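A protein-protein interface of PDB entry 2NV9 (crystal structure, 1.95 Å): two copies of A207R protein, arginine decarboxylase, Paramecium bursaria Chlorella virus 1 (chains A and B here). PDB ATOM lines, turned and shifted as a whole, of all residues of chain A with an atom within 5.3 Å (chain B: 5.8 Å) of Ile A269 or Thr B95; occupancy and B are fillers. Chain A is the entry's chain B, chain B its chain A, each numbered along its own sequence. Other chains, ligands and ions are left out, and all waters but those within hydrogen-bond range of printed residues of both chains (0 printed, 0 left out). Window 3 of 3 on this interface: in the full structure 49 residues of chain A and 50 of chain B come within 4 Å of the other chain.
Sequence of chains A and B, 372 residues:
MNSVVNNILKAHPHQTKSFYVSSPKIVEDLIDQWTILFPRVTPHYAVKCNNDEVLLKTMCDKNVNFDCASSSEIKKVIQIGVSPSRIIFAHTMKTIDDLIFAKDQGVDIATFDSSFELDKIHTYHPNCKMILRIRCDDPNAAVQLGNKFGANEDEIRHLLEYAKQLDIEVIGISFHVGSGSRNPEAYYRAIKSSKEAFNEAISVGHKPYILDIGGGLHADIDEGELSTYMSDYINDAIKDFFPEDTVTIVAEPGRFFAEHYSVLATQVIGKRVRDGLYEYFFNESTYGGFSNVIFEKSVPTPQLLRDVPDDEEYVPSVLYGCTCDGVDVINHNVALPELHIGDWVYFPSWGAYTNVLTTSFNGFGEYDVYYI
NZ of Lys B120 is in hydrogen-bond range of O of Ile A269 (2.7 Å).
The backbone carbonyl oxygen (O) of Lys B94 is in hydrogen-bond range of the side-chain amino group (NZ) of Lys B120, 2.6 Å away.
N of Asp B98 lies within hydrogen-bond range of OG1 of Thr B95, 2.9 Å away.
The side-chain carboxylate (OE1) of Glu B117 lies within salt-bridge range of the side-chain amino group (NZ) of Lys B120.
The backbone NH (N) of Ile A269 is in hydrogen-bond range of the backbone carbonyl oxygen (O) of Phe A281 (2.8 Å).
N of Phe A281 sits at hydrogen-bond distance from O of Gly A270 (2.9 Å).
Among the printed residues, pairs that only touch across the chains: Ile A269 with Thr B95 (3.5 Å), Gly A270 with Met B93 (3.9 Å), Lys A271 with Met B93 (3.7 Å), Phe A281 with Met B93 (3.7 Å) and Ile A341 with Lys B120 (3.96 Å).
Of chain B, only Thr B95 (3.5 Å) and Lys B120 (2.7 Å) come within 4 Å of Ile A269.
Of the printed residues of chain A, Met B93 touches Gly A270, Lys A271 and Phe A281.
Printed residues of chain B within 4 Å of Gly A270: Met B93 (3.9 Å).
Of the printed residues of chain B, Phe A281 touches Met B93.
Printed residues of chain A within 4 Å of Lys B120: Ile A269 (2.7 Å) and Ile A341 (3.96 Å).
Phe A282 touches none of the printed residues of chain B.
Gly A342 touches none of the printed residues of chain B.
The nearest residue of chain B that does not touch Ile A269 is Lys B94 (4.1 Å).
The nearest residue of chain A that does not touch Thr B95 is Asn A283 (4.9 Å).
The nearest printed residue of chain B that does not touch Lys A271 is Glu B117 (4.7 Å).
Printed residues of chain B that touch a printed residue of chain A: Met B93, Thr B95 and Lys B120.
Hydrophobic or aromatic side chains of chain B within 4 Å of the printed part of chain A: Met B93.
Of the 11 printed residues of chain A, 5 touch a printed residue of chain B.
Hydrophobic or aromatic side chains of chain A within 4 Å of the printed part of chain B: Ile A269, Phe A281 and Ile A341.
Among the printed residues, 6 pairs touch across the chains.
No position is printed for both chains.
Of the 6 pairs that touch across the chains among the printed residues, none has its exchanged pair printed and touching as well.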
ATOM      1  N   GLN A 267     -11.299   1.350   6.891  1.00  0.00           N
ATOM      2  CA  GLN A 267     -11.396   0.349   5.817  1.00  0.00           C
ATOM      3  C   GLN A 267     -10.082  -0.373   5.579  1.00  0.00           C
ATOM      4  O   GLN A 267      -9.015   0.214   5.731  1.00  0.00           O
ATOM      5  CB  GLN A 267     -11.846   1.010   4.498  1.00  0.00           C
ATOM      6  CG  GLN A 267     -12.314   0.037   3.417  1.00  0.00           C
ATOM      7  CD  GLN A 267     -12.575   0.765   2.073  1.00  0.00           C
ATOM      8  OE1 GLN A 267     -11.800   1.626   1.658  1.00  0.00           O
ATOM      9  NE2 GLN A 267     -13.665   0.397   1.411  1.00  0.00           N
ATOM     10  N   VAL A 268     -10.194  -1.639   5.185  1.00  0.00           N
ATOM     11  CA  VAL A 268      -9.058  -2.434   4.732  1.00  0.00           C
ATOM     12  C   VAL A 268      -8.675  -1.964   3.308  1.00  0.00           C
ATOM     13  O   VAL A 268      -9.504  -2.068   2.388  1.00  0.00           O
ATOM     14  CB  VAL A 268      -9.406  -3.951   4.664  1.00  0.00           C
ATOM     15  CG1 VAL A 268      -8.211  -4.723   4.146  1.00  0.00           C
ATOM     16  CG2 VAL A 268      -9.891  -4.504   6.048  1.00  0.00           C
ATOM     17  N   ILE A 269      -7.473  -1.411   3.163  1.00  0.00           N
ATOM     18  CA  ILE A 269      -7.003  -0.872   1.877  1.00  0.00           C
ATOM     19  C   ILE A 269      -5.896  -1.720   1.254  1.00  0.00           C
ATOM     20  O   ILE A 269      -5.587  -1.588   0.085  1.00  0.00           O
ATOM     21  CB  ILE A 269      -6.575   0.624   2.007  1.00  0.00           C
ATOM     22  CG1 ILE A 269      -5.254   0.751   2.809  1.00  0.00           C
ATOM     23  CG2 ILE A 269      -7.725   1.449   2.606  1.00  0.00           C
ATOM     24  CD1 ILE A 269      -5.145   2.140   3.446  1.00  0.00           C
ATOM     25  N   GLY A 270      -5.325  -2.642   2.050  1.00  0.00           N
ATOM     26  CA  GLY A 270      -4.211  -3.459   1.584  1.00  0.00           C
ATOM     27  C   GLY A 270      -4.239  -4.783   2.312  1.00  0.00           C
ATOM     28  O   GLY A 270      -4.763  -4.874   3.451  1.00  0.00           O
ATOM     29  N   LYS A 271      -3.678  -5.806   1.666  1.00  0.00           N
ATOM     30  CA  LYS A 271      -3.696  -7.163   2.205  1.00  0.00           C
ATOM     31  C   LYS A 271      -2.428  -7.921   1.782  1.00  0.00           C
ATOM     32  O   LYS A 271      -1.898  -7.730   0.684  1.00  0.00           O
ATOM     33  CB  LYS A 271      -4.978  -7.886   1.765  1.00  0.00           C
ATOM     34  CG  LYS A 271      -5.230  -9.250   2.384  1.00  0.00           C
ATOM     35  CD  LYS A 271      -6.519  -9.863   1.862  1.00  0.00           C
ATOM     36  CE  LYS A 271      -6.705 -11.292   2.449  1.00  0.00           C
ATOM     37  NZ  LYS A 271      -8.031 -11.883   2.160  1.00  0.00           N
ATOM     38  N   PHE A 281      -3.780  -3.772   5.960  1.00  0.00           N
ATOM     39  CA  PHE A 281      -3.410  -2.388   6.131  1.00  0.00           C
ATOM     40  C   PHE A 281      -4.694  -1.573   6.054  1.00  0.00           C
ATOM     41  O   PHE A 281      -5.544  -1.821   5.191  1.00  0.00           O
ATOM     42  CB  PHE A 281      -2.427  -1.965   5.055  1.00  0.00           C
ATOM     43  CG  PHE A 281      -1.039  -2.447   5.281  1.00  0.00           C
ATOM     44  CD1 PHE A 281      -0.050  -1.575   5.691  1.00  0.00           C
ATOM     45  CD2 PHE A 281      -0.717  -3.799   5.098  1.00  0.00           C
ATOM     46  CE1 PHE A 281       1.241  -2.017   5.889  1.00  0.00           C
ATOM     47  CE2 PHE A 281       0.601  -4.266   5.347  1.00  0.00           C
ATOM     48  CZ  PHE A 281       1.568  -3.372   5.713  1.00  0.00           C
ATOM     49  N   PHE A 282      -4.830  -0.634   6.980  1.00  0.00           N
ATOM     50  CA  PHE A 282      -6.079   0.143   7.124  1.00  0.00           C
ATOM     51  C   PHE A 282      -5.823   1.595   6.753  1.00  0.00           C
ATOM     52  O   PHE A 282      -4.661   2.048   6.759  1.00  0.00           O
ATOM     53  CB  PHE A 282      -6.626   0.074   8.565  1.00  0.00           C
ATOM     54  CG  PHE A 282      -7.178  -1.256   8.928  1.00  0.00           C
ATOM     55  CD1 PHE A 282      -8.530  -1.536   8.791  1.00  0.00           C
ATOM     56  CD2 PHE A 282      -6.318  -2.279   9.354  1.00  0.00           C
ATOM     57  CE1 PHE A 282      -9.035  -2.800   9.119  1.00  0.00           C
ATOM     58  CE2 PHE A 282      -6.802  -3.546   9.660  1.00  0.00           C
ATOM     59  CZ  PHE A 282      -8.163  -3.805   9.536  1.00  0.00           C
ATOM     60  N   ASN A 283      -6.900   2.330   6.444  1.00  0.00           N
ATOM     61  CA  ASN A 283      -6.760   3.775   6.168  1.00  0.00           C
ATOM     62  C   ASN A 283      -6.776   4.618   7.458  1.00  0.00           C
ATOM     63  O   ASN A 283      -7.267   5.767   7.492  1.00  0.00           O
ATOM     64  CB  ASN A 283      -7.770   4.276   5.101  1.00  0.00           C
ATOM     65  CG  ASN A 283      -9.213   4.230   5.574  1.00  0.00           C
ATOM     66  OD1 ASN A 283      -9.521   3.701   6.649  1.00  0.00           O
ATOM     67  ND2 ASN A 283     -10.119   4.790   4.754  1.00  0.00           N
ATOM     68  N   CYS A 322      -1.503   2.724   8.098  1.00  0.00           N
ATOM     69  CA  CYS A 322      -1.238   3.063   6.684  1.00  0.00           C
ATOM     70  C   CYS A 322       0.108   3.773   6.453  1.00  0.00           C
ATOM     71  O   CYS A 322       0.517   3.916   5.296  1.00  0.00           O
ATOM     72  CB  CYS A 322      -2.403   3.884   6.077  1.00  0.00           C
ATOM     73  SG  CYS A 322      -2.711   5.384   7.015  1.00  0.00           S
ATOM     74  N   ILE A 341      -9.898  -6.458   0.992  1.00  0.00           N
ATOM     75  CA  ILE A 341      -9.762  -5.062   0.646  1.00  0.00           C
ATOM     76  C   ILE A 341     -11.167  -4.540   0.327  1.00  0.00           C
ATOM     77  O   ILE A 341     -11.913  -5.173  -0.421  1.00  0.00           O
ATOM     78  CB  ILE A 341      -8.757  -4.901  -0.525  1.00  0.00           C
ATOM     79  CG1 ILE A 341      -7.361  -5.404  -0.083  1.00  0.00           C
ATOM     80  CG2 ILE A 341      -8.748  -3.464  -1.014  1.00  0.00           C
ATOM     81  CD1 ILE A 341      -6.290  -5.412  -1.152  1.00  0.00           C
ATOM     82  N   GLY A 342     -11.527  -3.420   0.958  1.00  0.00           N
ATOM     83  CA  GLY A 342     -12.858  -2.830   0.845  1.00  0.00           C
ATOM     84  C   GLY A 342     -13.731  -3.078   2.082  1.00  0.00           C
ATOM     85  O   GLY A 342     -14.715  -2.380   2.284  1.00  0.00           O
ATOM     86  N   MET B  93       1.746  -0.157   0.009  1.00  0.00           N
ATOM     87  CA  MET B  93       0.317  -0.335   0.237  1.00  0.00           C
ATOM     88  C   MET B  93      -0.393   0.997  -0.076  1.00  0.00           C
ATOM     89  O   MET B  93      -0.253   1.943   0.673  1.00  0.00           O
ATOM     90  CB  MET B  93       0.049  -0.773   1.667  1.00  0.00           C
ATOM     91  CG  MET B  93       0.561  -2.194   1.927  1.00  0.00           C
ATOM     92  SD  MET B  93      -0.386  -3.509   1.118  1.00  0.00           S
ATOM     93  CE  MET B  93       0.528  -5.042   1.656  1.00  0.00           C
ATOM     94  N   LYS B  94      -1.105   1.026  -1.208  1.00  0.00           N
ATOM     95  CA  LYS B  94      -1.720   2.251  -1.720  1.00  0.00           C
ATOM     96  C   LYS B  94      -3.222   2.054  -1.869  1.00  0.00           C
ATOM     97  O   LYS B  94      -3.677   1.051  -2.408  1.00  0.00           O
ATOM     98  CB  LYS B  94      -1.072   2.570  -3.084  1.00  0.00           C
ATOM     99  CG  LYS B  94       0.437   2.740  -2.992  1.00  0.00           C
ATOM    100  CD  LYS B  94       1.150   2.617  -4.356  1.00  0.00           C
ATOM    101  CE  LYS B  94       1.213   1.184  -4.891  1.00  0.00           C
ATOM    102  NZ  LYS B  94       1.837   0.156  -3.933  1.00  0.00           N
ATOM    103  N   THR B  95      -4.017   3.015  -1.438  1.00  0.00           N
ATOM    104  CA  THR B  95      -5.468   2.813  -1.570  1.00  0.00           C
ATOM    105  C   THR B  95      -5.844   2.746  -3.056  1.00  0.00           C
ATOM    106  O   THR B  95      -5.134   3.294  -3.895  1.00  0.00           O
ATOM    107  CB  THR B  95      -6.256   3.892  -0.856  1.00  0.00           C
ATOM    108  OG1 THR B  95      -6.138   5.100  -1.599  1.00  0.00           O
ATOM    109  CG2 THR B  95      -5.716   4.104   0.631  1.00  0.00           C
ATOM    110  N   ILE B  96      -6.933   2.039  -3.352  1.00  0.00           N
ATOM    111  CA  ILE B  96      -7.541   2.069  -4.703  1.00  0.00           C
ATOM    112  C   ILE B  96      -7.717   3.507  -5.226  1.00  0.00           C
ATOM    113  O   ILE B  96      -7.348   3.799  -6.357  1.00  0.00           O
ATOM    114  CB  ILE B  96      -8.857   1.259  -4.759  1.00  0.00           C
ATOM    115  CG1 ILE B  96      -8.499  -0.231  -4.743  1.00  0.00           C
ATOM    116  CG2 ILE B  96      -9.674   1.567  -6.018  1.00  0.00           C
ATOM    117  CD1 ILE B  96      -9.645  -1.112  -4.296  1.00  0.00           C
ATOM    118  N   ASP B  97      -8.261   4.390  -4.410  1.00  0.00           N
ATOM    119  CA  ASP B  97      -8.512   5.765  -4.880  1.00  0.00           C
ATOM    120  C   ASP B  97      -7.231   6.594  -5.064  1.00  0.00           C
ATOM    121  O   ASP B  97      -7.163   7.446  -5.938  1.00  0.00           O
ATOM    122  CB  ASP B  97      -9.528   6.483  -4.004  1.00  0.00           C
ATOM    123  CG  ASP B  97     -10.933   5.857  -4.105  1.00  0.00           C
ATOM    124  OD1 ASP B  97     -11.510   5.820  -5.212  1.00  0.00           O
ATOM    125  OD2 ASP B  97     -11.462   5.387  -3.070  1.00  0.00           O
ATOM    126  N   ASP B  98      -6.198   6.308  -4.272  1.00  0.00           N
ATOM    127  CA  ASP B  98      -4.898   6.948  -4.510  1.00  0.00           C
ATOM    128  C   ASP B  98      -4.250   6.435  -5.817  1.00  0.00           C
ATOM    129  O   ASP B  98      -3.561   7.186  -6.520  1.00  0.00           O
ATOM    130  CB  ASP B  98      -3.931   6.742  -3.326  1.00  0.00           C
ATOM    131  CG  ASP B  98      -4.223   7.685  -2.145  1.00  0.00           C
ATOM    132  OD1 ASP B  98      -5.297   8.332  -2.129  1.00  0.00           O
ATOM    133  OD2 ASP B  98      -3.371   7.747  -1.230  1.00  0.00           O
ATOM    134  N   LEU B  99      -4.405   5.130  -6.071  1.00  0.00           N
ATOM    135  CA  LEU B  99      -3.950   4.513  -7.320  1.00  0.00           C
ATOM    136  C   LEU B  99      -4.611   5.145  -8.579  1.00  0.00           C
ATOM    137  O   LEU B  99      -3.924   5.455  -9.544  1.00  0.00           O
ATOM    138  CB  LEU B  99      -4.231   3.011  -7.274  1.00  0.00           C
ATOM    139  CG  LEU B  99      -3.042   2.024  -7.071  1.00  0.00           C
ATOM    140  CD1 LEU B  99      -1.781   2.662  -6.549  1.00  0.00           C
ATOM    141  CD2 LEU B  99      -3.417   0.756  -6.264  1.00  0.00           C
ATOM    142  N   ILE B 100      -5.932   5.309  -8.538  1.00  0.00           N
ATOM    143  CA  ILE B 100      -6.711   5.991  -9.633  1.00  0.00           C
ATOM    144  C   ILE B 100      -6.220   7.440  -9.850  1.00  0.00           C
ATOM    145  O   ILE B 100      -5.964   7.858 -10.992  1.00  0.00           O
ATOM    146  CB  ILE B 100      -8.253   5.926  -9.408  1.00  0.00           C
ATOM    147  CG1 ILE B 100      -8.735   4.468  -9.298  1.00  0.00           C
ATOM    148  CG2 ILE B 100      -9.022   6.615 -10.565  1.00  0.00           C
ATOM    149  CD1 ILE B 100     -10.109   4.289  -8.723  1.00  0.00           C
ATOM    150  N   GLU B 117      -1.564  -6.440  -3.827  1.00  0.00           N
ATOM    151  CA  GLU B 117      -1.210  -5.129  -4.326  1.00  0.00           C
ATOM    152  C   GLU B 117      -1.163  -5.164  -5.861  1.00  0.00           C
ATOM    153  O   GLU B 117      -1.518  -4.199  -6.504  1.00  0.00           O
ATOM    154  CB  GLU B 117       0.120  -4.627  -3.791  1.00  0.00           C
ATOM    155  CG  GLU B 117       0.302  -3.094  -3.952  1.00  0.00           C
ATOM    156  CD  GLU B 117      -0.598  -2.239  -3.000  1.00  0.00           C
ATOM    157  OE1 GLU B 117      -1.261  -2.810  -2.079  1.00  0.00           O
ATOM    158  OE2 GLU B 117      -0.573  -0.978  -3.129  1.00  0.00           O
ATOM    159  N   LYS B 120      -4.675  -5.044  -7.334  1.00  0.00           N
ATOM    160  CA  LYS B 120      -5.082  -3.632  -7.349  1.00  0.00           C
ATOM    161  C   LYS B 120      -4.508  -2.862  -8.557  1.00  0.00           C
ATOM    162  O   LYS B 120      -5.236  -2.139  -9.261  1.00  0.00           O
ATOM    163  CB  LYS B 120      -4.651  -2.965  -6.050  1.00  0.00           C
ATOM    164  CG  LYS B 120      -5.675  -3.080  -4.944  1.00  0.00           C
ATOM    165  CD  LYS B 120      -5.380  -2.085  -3.790  1.00  0.00           C
ATOM    166  CE  LYS B 120      -4.229  -2.553  -2.957  1.00  0.00           C
ATOM    167  NZ  LYS B 120      -3.816  -1.544  -1.919  1.00  0.00           N
